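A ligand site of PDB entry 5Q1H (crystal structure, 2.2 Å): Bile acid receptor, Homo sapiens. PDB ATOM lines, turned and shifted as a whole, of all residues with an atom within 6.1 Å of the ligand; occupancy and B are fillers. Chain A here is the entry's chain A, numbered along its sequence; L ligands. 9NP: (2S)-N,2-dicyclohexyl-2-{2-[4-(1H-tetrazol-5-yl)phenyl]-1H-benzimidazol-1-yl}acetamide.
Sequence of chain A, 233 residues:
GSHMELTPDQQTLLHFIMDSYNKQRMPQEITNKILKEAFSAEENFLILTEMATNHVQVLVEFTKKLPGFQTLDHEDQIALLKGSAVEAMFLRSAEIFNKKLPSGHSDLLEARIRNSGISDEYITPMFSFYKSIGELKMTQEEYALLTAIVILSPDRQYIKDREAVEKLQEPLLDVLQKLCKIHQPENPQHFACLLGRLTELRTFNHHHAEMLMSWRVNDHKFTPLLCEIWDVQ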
ATOM      1  N   ILE A  30      -8.056  11.479  12.303  1.00  0.00           N
ATOM      2  CA  ILE A  30      -7.015  12.462  12.603  1.00  0.00           C
ATOM      3  C   ILE A  30      -6.284  12.915  11.312  1.00  0.00           C
ATOM      4  O   ILE A  30      -6.161  14.118  11.082  1.00  0.00           O
ATOM      5  CB  ILE A  30      -6.060  11.816  13.655  1.00  0.00           C
ATOM      6  CG1 ILE A  30      -6.854  11.437  14.945  1.00  0.00           C
ATOM      7  CG2 ILE A  30      -4.831  12.681  13.938  1.00  0.00           C
ATOM      8  CD1 ILE A  30      -6.308  10.300  15.764  1.00  0.00           C
ATOM      9  N   THR A  31      -5.762  11.963  10.508  1.00  0.00           N
ATOM     10  CA  THR A  31      -5.030  12.285   9.271  1.00  0.00           C
ATOM     11  C   THR A  31      -5.926  12.867   8.163  1.00  0.00           C
ATOM     12  O   THR A  31      -5.447  13.743   7.453  1.00  0.00           O
ATOM     13  CB  THR A  31      -4.206  11.106   8.757  1.00  0.00           C
ATOM     14  OG1 THR A  31      -5.065  10.009   8.486  1.00  0.00           O
ATOM     15  CG2 THR A  31      -3.126  10.692   9.735  1.00  0.00           C
ATOM     16  N   ILE A  34      -6.171  16.672   8.808  1.00  0.00           N
ATOM     17  CA  ILE A  34      -4.853  17.274   8.539  1.00  0.00           C
ATOM     18  C   ILE A  34      -4.550  17.324   7.048  1.00  0.00           C
ATOM     19  O   ILE A  34      -4.060  18.344   6.574  1.00  0.00           O
ATOM     20  CB  ILE A  34      -3.716  16.552   9.347  1.00  0.00           C
ATOM     21  CG1 ILE A  34      -3.873  16.784  10.843  1.00  0.00           C
ATOM     22  CG2 ILE A  34      -2.323  17.013   8.881  1.00  0.00           C
ATOM     23  CD1 ILE A  34      -3.139  15.724  11.720  1.00  0.00           C
ATOM     24  N   ASN A  44      -4.263  25.004  14.206  1.00  0.00           N
ATOM     25  CA  ASN A  44      -3.618  23.724  14.503  1.00  0.00           C
ATOM     26  C   ASN A  44      -3.401  23.538  15.980  1.00  0.00           C
ATOM     27  O   ASN A  44      -3.428  22.407  16.449  1.00  0.00           O
ATOM     28  CB  ASN A  44      -2.272  23.599  13.794  1.00  0.00           C
ATOM     29  CG  ASN A  44      -2.386  23.380  12.309  1.00  0.00           C
ATOM     30  OD1 ASN A  44      -3.204  22.604  11.824  1.00  0.00           O
ATOM     31  ND2 ASN A  44      -1.514  24.029  11.563  1.00  0.00           N
ATOM     32  N   PHE A  45      -3.198  24.637  16.712  1.00  0.00           N
ATOM     33  CA  PHE A  45      -2.972  24.597  18.164  1.00  0.00           C
ATOM     34  C   PHE A  45      -4.271  24.204  18.847  1.00  0.00           C
ATOM     35  O   PHE A  45      -4.254  23.375  19.768  1.00  0.00           O
ATOM     36  CB  PHE A  45      -2.439  25.936  18.696  1.00  0.00           C
ATOM     37  CG  PHE A  45      -2.050  25.849  20.150  1.00  0.00           C
ATOM     38  CD1 PHE A  45      -0.828  25.314  20.526  1.00  0.00           C
ATOM     39  CD2 PHE A  45      -2.930  26.274  21.150  1.00  0.00           C
ATOM     40  CE1 PHE A  45      -0.484  25.216  21.880  1.00  0.00           C
ATOM     41  CE2 PHE A  45      -2.576  26.175  22.495  1.00  0.00           C
ATOM     42  CZ  PHE A  45      -1.366  25.636  22.858  1.00  0.00           C
ATOM     43  N   ILE A  47      -6.693  22.419  17.293  1.00  0.00           N
ATOM     44  CA  ILE A  47      -6.855  20.989  16.944  1.00  0.00           C
ATOM     45  C   ILE A  47      -6.024  20.116  17.896  1.00  0.00           C
ATOM     46  O   ILE A  47      -6.558  19.182  18.512  1.00  0.00           O
ATOM     47  CB  ILE A  47      -6.508  20.725  15.446  1.00  0.00           C
ATOM     48  CG1 ILE A  47      -7.565  21.371  14.534  1.00  0.00           C
ATOM     49  CG2 ILE A  47      -6.336  19.210  15.161  1.00  0.00           C
ATOM     50  CD1 ILE A  47      -7.099  21.670  13.100  1.00  0.00           C
ATOM     51  N   LEU A  48      -4.739  20.468  18.101  1.00  0.00           N
ATOM     52  CA  LEU A  48      -3.917  19.723  19.073  1.00  0.00           C
ATOM     53  C   LEU A  48      -4.585  19.658  20.477  1.00  0.00           C
ATOM     54  O   LEU A  48      -4.679  18.578  21.046  1.00  0.00           O
ATOM     55  CB  LEU A  48      -2.507  20.354  19.207  1.00  0.00           C
ATOM     56  CG  LEU A  48      -1.624  19.738  20.336  1.00  0.00           C
ATOM     57  CD1 LEU A  48      -1.283  18.252  20.051  1.00  0.00           C
ATOM     58  CD2 LEU A  48      -0.331  20.499  20.531  1.00  0.00           C
ATOM     59  N   MET A  51      -7.562  17.337  20.429  1.00  0.00           N
ATOM     60  CA  MET A  51      -7.067  15.960  20.235  1.00  0.00           C
ATOM     61  C   MET A  51      -6.491  15.412  21.527  1.00  0.00           C
ATOM     62  O   MET A  51      -6.765  14.262  21.912  1.00  0.00           O
ATOM     63  CB  MET A  51      -5.963  15.900  19.150  1.00  0.00           C
ATOM     64  CG  MET A  51      -6.452  16.139  17.732  1.00  0.00           C
ATOM     65  SD  MET A  51      -7.630  14.900  17.114  1.00  0.00           S
ATOM     66  CE  MET A  51      -6.695  13.503  17.327  1.00  0.00           C
ATOM     67  N   ALA A  52      -5.657  16.246  22.210  1.00  0.00           N
ATOM     68  CA  ALA A  52      -5.022  15.827  23.449  1.00  0.00           C
ATOM     69  C   ALA A  52      -6.008  15.659  24.567  1.00  0.00           C
ATOM     70  O   ALA A  52      -5.765  14.819  25.430  1.00  0.00           O
ATOM     71  CB  ALA A  52      -3.945  16.804  23.870  1.00  0.00           C
ATOM     72  N   HIS A  55      -7.658  12.430  23.966  1.00  0.00           N
ATOM     73  CA  HIS A  55      -6.684  11.371  24.199  1.00  0.00           C
ATOM     74  C   HIS A  55      -6.525  11.023  25.691  1.00  0.00           C
ATOM     75  O   HIS A  55      -6.536   9.849  26.058  1.00  0.00           O
ATOM     76  CB  HIS A  55      -5.291  11.739  23.639  1.00  0.00           C
ATOM     77  CG  HIS A  55      -4.262  10.724  23.988  1.00  0.00           C
ATOM     78  ND1 HIS A  55      -3.324  10.960  24.981  1.00  0.00           N
ATOM     79  CD2 HIS A  55      -4.086   9.477  23.506  1.00  0.00           C
ATOM     80  CE1 HIS A  55      -2.590   9.867  25.055  1.00  0.00           C
ATOM     81  NE2 HIS A  55      -3.007   8.945  24.183  1.00  0.00           N
ATOM     82  N   ALA A  88       2.394   8.699  26.371  1.00  0.00           N
ATOM     83  CA  ALA A  88       1.332   7.970  25.633  1.00  0.00           C
ATOM     84  C   ALA A  88       0.830   8.794  24.435  1.00  0.00           C
ATOM     85  O   ALA A  88       0.559   8.224  23.385  1.00  0.00           O
ATOM     86  CB  ALA A  88       0.191   7.618  26.552  1.00  0.00           C
ATOM     87  N   MET A  89       0.767  10.144  24.572  1.00  0.00           N
ATOM     88  CA  MET A  89       0.326  10.980  23.427  1.00  0.00           C
ATOM     89  C   MET A  89       1.325  10.903  22.285  1.00  0.00           C
ATOM     90  O   MET A  89       0.913  10.771  21.137  1.00  0.00           O
ATOM     91  CB  MET A  89       0.039  12.428  23.835  1.00  0.00           C
ATOM     92  CG  MET A  89       0.226  13.440  22.679  1.00  0.00           C
ATOM     93  SD  MET A  89      -0.047  15.152  23.128  1.00  0.00           S
ATOM     94  CE  MET A  89       1.567  15.528  23.886  1.00  0.00           C
ATOM     95  N   PHE A  90       2.635  10.990  22.591  1.00  0.00           N
ATOM     96  CA  PHE A  90       3.655  10.910  21.553  1.00  0.00           C
ATOM     97  C   PHE A  90       3.759   9.493  20.928  1.00  0.00           C
ATOM     98  O   PHE A  90       3.999   9.373  19.728  1.00  0.00           O
ATOM     99  CB  PHE A  90       5.001  11.406  22.076  1.00  0.00           C
ATOM    100  CG  PHE A  90       5.077  12.925  22.088  1.00  0.00           C
ATOM    101  CD1 PHE A  90       5.071  13.644  20.899  1.00  0.00           C
ATOM    102  CD2 PHE A  90       5.218  13.611  23.279  1.00  0.00           C
ATOM    103  CE1 PHE A  90       5.166  15.043  20.910  1.00  0.00           C
ATOM    104  CE2 PHE A  90       5.303  15.011  23.300  1.00  0.00           C
ATOM    105  CZ  PHE A  90       5.295  15.713  22.110  1.00  0.00           C
ATOM    106  N   ARG A  92       1.175   7.311  20.664  1.00  0.00           N
ATOM    107  CA  ARG A  92      -0.010   7.208  19.789  1.00  0.00           C
ATOM    108  C   ARG A  92       0.161   8.059  18.506  1.00  0.00           C
ATOM    109  O   ARG A  92      -0.242   7.637  17.426  1.00  0.00           O
ATOM    110  CB  ARG A  92      -1.295   7.602  20.558  1.00  0.00           C
ATOM    111  CG  ARG A  92      -2.536   7.673  19.638  1.00  0.00           C
ATOM    112  CD  ARG A  92      -2.903   6.253  19.206  1.00  0.00           C
ATOM    113  NE  ARG A  92      -4.158   6.222  18.477  1.00  0.00           N
ATOM    114  CZ  ARG A  92      -4.704   5.129  17.968  1.00  0.00           C
ATOM    115  NH1 ARG A  92      -4.088   3.964  18.070  1.00  0.00           N
ATOM    116  NH2 ARG A  92      -5.861   5.202  17.334  1.00  0.00           N
ATOM    117  N   SER A  93       0.760   9.265  18.627  1.00  0.00           N
ATOM    118  CA  SER A  93       1.015  10.105  17.455  1.00  0.00           C
ATOM    119  C   SER A  93       1.976   9.394  16.485  1.00  0.00           C
ATOM    120  O   SER A  93       1.810   9.506  15.266  1.00  0.00           O
ATOM    121  CB  SER A  93       1.634  11.438  17.873  1.00  0.00           C
ATOM    122  OG  SER A  93       0.857  12.161  18.810  1.00  0.00           O
ATOM    123  N   ALA A  94       2.985   8.692  17.032  1.00  0.00           N
ATOM    124  CA  ALA A  94       4.004   7.946  16.220  1.00  0.00           C
ATOM    125  C   ALA A  94       3.321   6.802  15.499  1.00  0.00           C
ATOM    126  O   ALA A  94       3.671   6.500  14.360  1.00  0.00           O
ATOM    127  CB  ALA A  94       5.116   7.386  17.121  1.00  0.00           C
ATOM    128  N   ILE A  96       0.107   6.718  14.547  1.00  0.00           N
ATOM    129  CA  ILE A  96      -0.669   7.378  13.506  1.00  0.00           C
ATOM    130  C   ILE A  96       0.227   7.789  12.363  1.00  0.00           C
ATOM    131  O   ILE A  96      -0.033   7.402  11.225  1.00  0.00           O
ATOM    132  CB  ILE A  96      -1.535   8.538  14.050  1.00  0.00           C
ATOM    133  CG1 ILE A  96      -2.565   8.008  15.053  1.00  0.00           C
ATOM    134  CG2 ILE A  96      -2.231   9.310  12.899  1.00  0.00           C
ATOM    135  CD1 ILE A  96      -3.004   9.004  16.002  1.00  0.00           C
ATOM    136  N   PHE A  97       1.304   8.510  12.654  1.00  0.00           N
ATOM    137  CA  PHE A  97       2.267   8.950  11.651  1.00  0.00           C
ATOM    138  C   PHE A  97       2.739   7.824  10.749  1.00  0.00           C
ATOM    139  O   PHE A  97       2.849   8.008   9.546  1.00  0.00           O
ATOM    140  CB  PHE A  97       3.483   9.613  12.342  1.00  0.00           C
ATOM    141  CG  PHE A  97       4.421  10.226  11.338  1.00  0.00           C
ATOM    142  CD1 PHE A  97       4.071  11.396  10.681  1.00  0.00           C
ATOM    143  CD2 PHE A  97       5.585   9.571  10.959  1.00  0.00           C
ATOM    144  CE1 PHE A  97       4.895  11.925   9.688  1.00  0.00           C
ATOM    145  CE2 PHE A  97       6.421  10.103   9.979  1.00  0.00           C
ATOM    146  CZ  PHE A  97       6.075  11.276   9.357  1.00  0.00           C
ATOM    147  N   LEU A 109       1.501  14.584   5.004  1.00  0.00           N
ATOM    148  CA  LEU A 109       1.287  14.506   6.457  1.00  0.00           C
ATOM    149  C   LEU A 109       2.492  15.088   7.165  1.00  0.00           C
ATOM    150  O   LEU A 109       2.325  15.983   7.978  1.00  0.00           O
ATOM    151  CB  LEU A 109       1.001  13.054   6.950  1.00  0.00           C
ATOM    152  CG  LEU A 109       0.539  12.932   8.434  1.00  0.00           C
ATOM    153  CD1 LEU A 109      -0.840  13.545   8.640  1.00  0.00           C
ATOM    154  CD2 LEU A 109       0.573  11.488   8.936  1.00  0.00           C
ATOM    155  N   ARG A 112       2.666  18.850   6.554  1.00  0.00           N
ATOM    156  CA  ARG A 112       1.635  19.510   7.361  1.00  0.00           C
ATOM    157  C   ARG A 112       2.046  19.619   8.820  1.00  0.00           C
ATOM    158  O   ARG A 112       1.887  20.701   9.407  1.00  0.00           O
ATOM    159  CB  ARG A 112       0.281  18.814   7.208  1.00  0.00           C
ATOM    160  CG  ARG A 112      -0.340  18.988   5.821  1.00  0.00           C
ATOM    161  CD  ARG A 112      -1.325  20.139   5.744  1.00  0.00           C
ATOM    162  NE  ARG A 112      -1.468  20.625   4.370  1.00  0.00           N
ATOM    163  CZ  ARG A 112      -2.410  20.212   3.522  1.00  0.00           C
ATOM    164  NH1 ARG A 112      -3.344  19.346   3.914  1.00  0.00           N
ATOM    165  NH2 ARG A 112      -2.454  20.688   2.285  1.00  0.00           N
ATOM    166  N   ILE A 113       2.653  18.536   9.368  1.00  0.00           N
ATOM    167  CA  ILE A 113       3.155  18.531  10.738  1.00  0.00           C
ATOM    168  C   ILE A 113       4.369  19.464  10.884  1.00  0.00           C
ATOM    169  O   ILE A 113       4.403  20.248  11.839  1.00  0.00           O
ATOM    170  CB  ILE A 113       3.395  17.113  11.311  1.00  0.00           C
ATOM    171  CG1 ILE A 113       2.099  16.290  11.294  1.00  0.00           C
ATOM    172  CG2 ILE A 113       3.909  17.191  12.736  1.00  0.00           C
ATOM    173  CD1 ILE A 113       2.353  14.818  11.401  1.00  0.00           C
ATOM    174  N   SER A 116       3.014  23.089  10.906  1.00  0.00           N
ATOM    175  CA  SER A 116       1.824  23.268  11.745  1.00  0.00           C
ATOM    176  C   SER A 116       1.848  24.461  12.722  1.00  0.00           C
ATOM    177  O   SER A 116       0.784  24.956  13.108  1.00  0.00           O
ATOM    178  CB  SER A 116       1.519  21.985  12.511  1.00  0.00           C
ATOM    179  OG  SER A 116       2.571  21.684  13.418  1.00  0.00           O
ATOM    180  N   ILE A 118       4.589  24.200  15.323  1.00  0.00           N
ATOM    181  CA  ILE A 118       5.610  23.715  16.265  1.00  0.00           C
ATOM    182  C   ILE A 118       6.929  24.400  15.865  1.00  0.00           C
ATOM    183  O   ILE A 118       7.181  24.558  14.671  1.00  0.00           O
ATOM    184  CB  ILE A 118       5.772  22.162  16.189  1.00  0.00           C
ATOM    185  CG1 ILE A 118       4.417  21.423  16.288  1.00  0.00           C
ATOM    186  CG2 ILE A 118       6.782  21.654  17.256  1.00  0.00           C
ATOM    187  CD1 ILE A 118       4.414  19.952  15.740  1.00  0.00           C
ATOM    188  N   MET A 126      11.159  15.178  17.555  1.00  0.00           N
ATOM    189  CA  MET A 126       9.838  14.600  17.303  1.00  0.00           C
ATOM    190  C   MET A 126       9.860  13.683  16.069  1.00  0.00           C
ATOM    191  O   MET A 126       9.433  12.529  16.169  1.00  0.00           O
ATOM    192  CB  MET A 126       8.751  15.681  17.154  1.00  0.00           C
ATOM    193  CG  MET A 126       7.324  15.142  17.199  1.00  0.00           C
ATOM    194  SD  MET A 126       6.041  16.371  16.788  1.00  0.00           S
ATOM    195  CE  MET A 126       6.415  16.688  15.151  1.00  0.00           C
ATOM    196  N   TYR A 130       9.560   9.452  15.526  1.00  0.00           N
ATOM    197  CA  TYR A 130       8.551   8.888  14.623  1.00  0.00           C
ATOM    198  C   TYR A 130       9.179   7.969  13.608  1.00  0.00           C
ATOM    199  O   TYR A 130       8.603   6.915  13.313  1.00  0.00           O
ATOM    200  CB  TYR A 130       7.731   9.988  13.899  1.00  0.00           C
ATOM    201  CG  TYR A 130       6.794  10.848  14.746  1.00  0.00           C
ATOM    202  CD1 TYR A 130       6.604  10.585  16.098  1.00  0.00           C
ATOM    203  CD2 TYR A 130       6.117  11.931  14.185  1.00  0.00           C
ATOM    204  CE1 TYR A 130       5.752  11.374  16.875  1.00  0.00           C
ATOM    205  CE2 TYR A 130       5.235  12.706  14.953  1.00  0.00           C
ATOM    206  CZ  TYR A 130       5.067  12.423  16.299  1.00  0.00           C
ATOM    207  OH  TYR A 130       4.234  13.210  17.057  1.00  0.00           O
ATOM    208  N   HIS A 208       8.396  19.162  27.597  1.00  0.00           N
ATOM    209  CA  HIS A 208       7.019  19.310  27.114  1.00  0.00           C
ATOM    210  C   HIS A 208       6.417  20.702  27.327  1.00  0.00           C
ATOM    211  O   HIS A 208       5.916  21.285  26.370  1.00  0.00           O
ATOM    212  CB  HIS A 208       6.100  18.250  27.705  1.00  0.00           C
ATOM    213  CG  HIS A 208       4.757  18.275  27.043  1.00  0.00           C
ATOM    214  ND1 HIS A 208       4.632  18.157  25.672  1.00  0.00           N
ATOM    215  CD2 HIS A 208       3.532  18.463  27.585  1.00  0.00           C
ATOM    216  CE1 HIS A 208       3.333  18.222  25.434  1.00  0.00           C
ATOM    217  NE2 HIS A 208       2.643  18.421  26.553  1.00  0.00           N
ATOM    218  N   MET A 211       8.039  23.012  24.814  1.00  0.00           N
ATOM    219  CA  MET A 211       7.599  22.715  23.455  1.00  0.00           C
ATOM    220  C   MET A 211       6.215  23.376  23.207  1.00  0.00           C
ATOM    221  O   MET A 211       6.041  24.035  22.176  1.00  0.00           O
ATOM    222  CB  MET A 211       7.524  21.190  23.239  1.00  0.00           C
ATOM    223  CG  MET A 211       6.934  20.778  21.919  1.00  0.00           C
ATOM    224  SD  MET A 211       7.043  18.990  21.675  1.00  0.00           S
ATOM    225  CE  MET A 211       6.501  18.881  20.006  1.00  0.00           C
ATOM    226  N   LEU A 212       5.285  23.267  24.173  1.00  0.00           N
ATOM    227  CA  LEU A 212       3.950  23.844  24.067  1.00  0.00           C
ATOM    228  C   LEU A 212       3.962  25.359  23.969  1.00  0.00           C
ATOM    229  O   LEU A 212       3.250  25.901  23.122  1.00  0.00           O
ATOM    230  CB  LEU A 212       3.079  23.463  25.243  1.00  0.00           C
ATOM    231  CG  LEU A 212       2.639  22.036  25.344  1.00  0.00           C
ATOM    232  CD1 LEU A 212       2.250  21.749  26.797  1.00  0.00           C
ATOM    233  CD2 LEU A 212       1.526  21.743  24.356  1.00  0.00           C
ATOM    234  N   TRP A 215       5.149  27.070  20.492  1.00  0.00           N
ATOM    235  CA  TRP A 215       4.293  26.979  19.304  1.00  0.00           C
ATOM    236  C   TRP A 215       4.092  28.441  18.820  1.00  0.00           C
ATOM    237  O   TRP A 215       3.914  29.337  19.643  1.00  0.00           O
ATOM    238  CB  TRP A 215       2.947  26.381  19.688  1.00  0.00           C
ATOM    239  CG  TRP A 215       2.752  24.927  19.339  1.00  0.00           C
ATOM    240  CD1 TRP A 215       3.204  23.845  20.053  1.00  0.00           C
ATOM    241  CD2 TRP A 215       1.945  24.408  18.284  1.00  0.00           C
ATOM    242  NE1 TRP A 215       2.731  22.680  19.485  1.00  0.00           N
ATOM    243  CE2 TRP A 215       1.955  23.005  18.394  1.00  0.00           C
ATOM    244  CE3 TRP A 215       1.225  24.998  17.217  1.00  0.00           C
ATOM    245  CZ2 TRP A 215       1.263  22.176  17.490  1.00  0.00           C
ATOM    246  CZ3 TRP A 215       0.553  24.182  16.332  1.00  0.00           C
ATOM    247  CH2 TRP A 215       0.586  22.787  16.466  1.00  0.00           C
ATOM    248  N   TRP A 230      -0.608  18.608  31.971  1.00  0.00           N
ATOM    249  CA  TRP A 230       0.592  19.164  31.353  1.00  0.00           C
ATOM    250  C   TRP A 230       1.318  20.213  32.210  1.00  0.00           C
ATOM    251  O   TRP A 230       2.387  20.675  31.804  1.00  0.00           O
ATOM    252  CB  TRP A 230       0.208  19.786  30.010  1.00  0.00           C
ATOM    253  CG  TRP A 230      -0.137  18.826  28.907  1.00  0.00           C
ATOM    254  CD1 TRP A 230       0.085  17.477  28.886  1.00  0.00           C
ATOM    255  CD2 TRP A 230      -0.681  19.170  27.626  1.00  0.00           C
ATOM    256  NE1 TRP A 230      -0.274  16.969  27.665  1.00  0.00           N
ATOM    257  CE2 TRP A 230      -0.736  17.981  26.874  1.00  0.00           C
ATOM    258  CE3 TRP A 230      -1.058  20.387  27.031  1.00  0.00           C
ATOM    259  CZ2 TRP A 230      -1.164  17.967  25.544  1.00  0.00           C
ATOM    260  CZ3 TRP A 230      -1.515  20.370  25.721  1.00  0.00           C
ATOM    261  CH2 TRP A 230      -1.553  19.178  24.987  1.00  0.00           C
HETATM  262  N3  9NP L   1       2.107  14.331  15.853  1.00  0.00           N
HETATM  263  C4  9NP L   1      -2.126  15.553  16.889  1.00  0.00           C
HETATM  264  C8  9NP L   1       2.893  18.764  20.662  1.00  0.00           C
HETATM  265  C10 9NP L   1       0.028  14.294  14.881  1.00  0.00           C
HETATM  266  C15 9NP L   1       2.520  17.890  19.543  1.00  0.00           C
HETATM  267  C17 9NP L   1       1.686  15.768  18.743  1.00  0.00           C
HETATM  268  C20 9NP L   1       2.048  16.594  19.794  1.00  0.00           C
HETATM  269  C21 9NP L   1      -1.355  17.276  15.109  1.00  0.00           C
HETATM  270  C22 9NP L   1      -2.683  13.757  18.491  1.00  0.00           C
HETATM  271  C24 9NP L   1       1.543  12.615  14.073  1.00  0.00           C
HETATM  272  C26 9NP L   1      -2.094  18.486  15.679  1.00  0.00           C
HETATM  273  C28 9NP L   1      -2.627  12.313  17.961  1.00  0.00           C
HETATM  274  O16 9NP L   1      -3.290  15.828  16.631  1.00  0.00           O
HETATM  275  N13 9NP L   1      -1.765  14.598  17.744  1.00  0.00           N
HETATM  276  C34 9NP L   1      -3.547  11.374  18.788  1.00  0.00           C
HETATM  277  C35 9NP L   1      -3.203  11.431  20.294  1.00  0.00           C
HETATM  278  C33 9NP L   1      -3.268  12.848  20.816  1.00  0.00           C
HETATM  279  C27 9NP L   1      -2.340  13.810  19.975  1.00  0.00           C
HETATM  280  C9  9NP L   1      -0.967  16.297  16.232  1.00  0.00           C
HETATM  281  C31 9NP L   1      -2.554  19.451  14.564  1.00  0.00           C
HETATM  282  C36 9NP L   1      -1.364  19.956  13.733  1.00  0.00           C
HETATM  283  C32 9NP L   1      -0.507  18.773  13.204  1.00  0.00           C
HETATM  284  C25 9NP L   1      -0.122  17.783  14.334  1.00  0.00           C
HETATM  285  N2  9NP L   1       0.101  15.323  15.833  1.00  0.00           N
HETATM  286  C23 9NP L   1      -0.983  13.856  14.025  1.00  0.00           C
HETATM  287  C29 9NP L   1      -0.703  12.788  13.193  1.00  0.00           C
HETATM  288  C30 9NP L   1       0.542  12.176  13.207  1.00  0.00           C
HETATM  289  C12 9NP L   1       1.278  13.698  14.910  1.00  0.00           C
HETATM  290  C1  9NP L   1       1.360  15.282  16.366  1.00  0.00           C
HETATM  291  C14 9NP L   1       1.787  16.205  17.426  1.00  0.00           C
HETATM  292  C18 9NP L   1       2.236  17.504  17.181  1.00  0.00           C
HETATM  293  C19 9NP L   1       2.600  18.325  18.224  1.00  0.00           C
HETATM  294  N7  9NP L   1       2.847  18.449  21.955  1.00  0.00           N
HETATM  295  N5  9NP L   1       3.255  19.509  22.681  1.00  0.00           N
HETATM  296  N6  9NP L   1       3.539  20.444  21.831  1.00  0.00           N
HETATM  297  N11 9NP L   1       3.322  20.018  20.556  1.00  0.00           N
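O of Ile 34 sits at hydrogen-bond distance from NH1 of Arg 112, 2.9 Å away.
The side-chain amide nitrogen (ND2) of Asn 44 lies within hydrogen-bond range of the backbone carbonyl oxygen (O) of Ser 116 (2.9 Å).
NE1 of Trp 230 sits close to NE2 of His 208.
OG of Ser 93 is in hydrogen-bond range of O of Met 89, 2.7 Å away.
OG of Ser 116 lies within hydrogen-bond range of O of Ile 113, at 2.8 Å.
The side-chain hydroxyl (OH) of Tyr 130 sits close to the side-chain sulfur (SD) of Met 126, 3.7 Å away.
The indole nitrogen of Trp 215 sits at hydrogen-bond distance from a nitrogen (N11) of the ligand, at 2.9 Å.
SD of Met 211 lies close to N6 of the ligand, 3.8 Å away.
The side-chain hydroxyl of Tyr 130 lies within hydrogen-bond range of a nitrogen (N3) of the ligand, at 2.7 Å.
Residues that only touch the ligand: His 208 (3.0 Å), Leu 212 (3.3 Å), Ser 93 (3.3 Å), Met 51 (3.4 Å), Ile 118 (3.5 Å), Ile 113 (3.6 Å), Asn 44 (3.6 Å), His 55 (3.6 Å), Phe 90 (3.7 Å), Leu 48 (3.7 Å), Ile 34 (3.7 Å), Ile 96 (3.7 Å), Met 89 (3.7 Å), Ser 116 (3.7 Å), Phe 97 (3.8 Å), Ile 47 (3.8 Å), Arg 92 (3.9 Å) and Met 126 (3.99 Å).
Hydrophobic or aromatic side chains within 4 Å of the ligand: Ile 34, Ile 47, Leu 48, Met 51, His 55, Met 89, Phe 90, Ile 96, Phe 97, Ile 113, Ile 118, Met 126, Tyr 130, His 208, Met 211, Leu 212 and Trp 215.
Within 4 Å of the ligand: Ile 34, Asn 44, Ile 47, Leu 48, Met 51, His 55, Met 89, Phe 90, Arg 92, Ser 93, Ile 96, Phe 97, Ile 113, Ser 116, Ile 118, Met 126, Tyr 130, His 208, Met 211, Leu 212 and Trp 215.
The nearest printed residue that does not touch the ligand is Ile 30 (4.02 Å).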
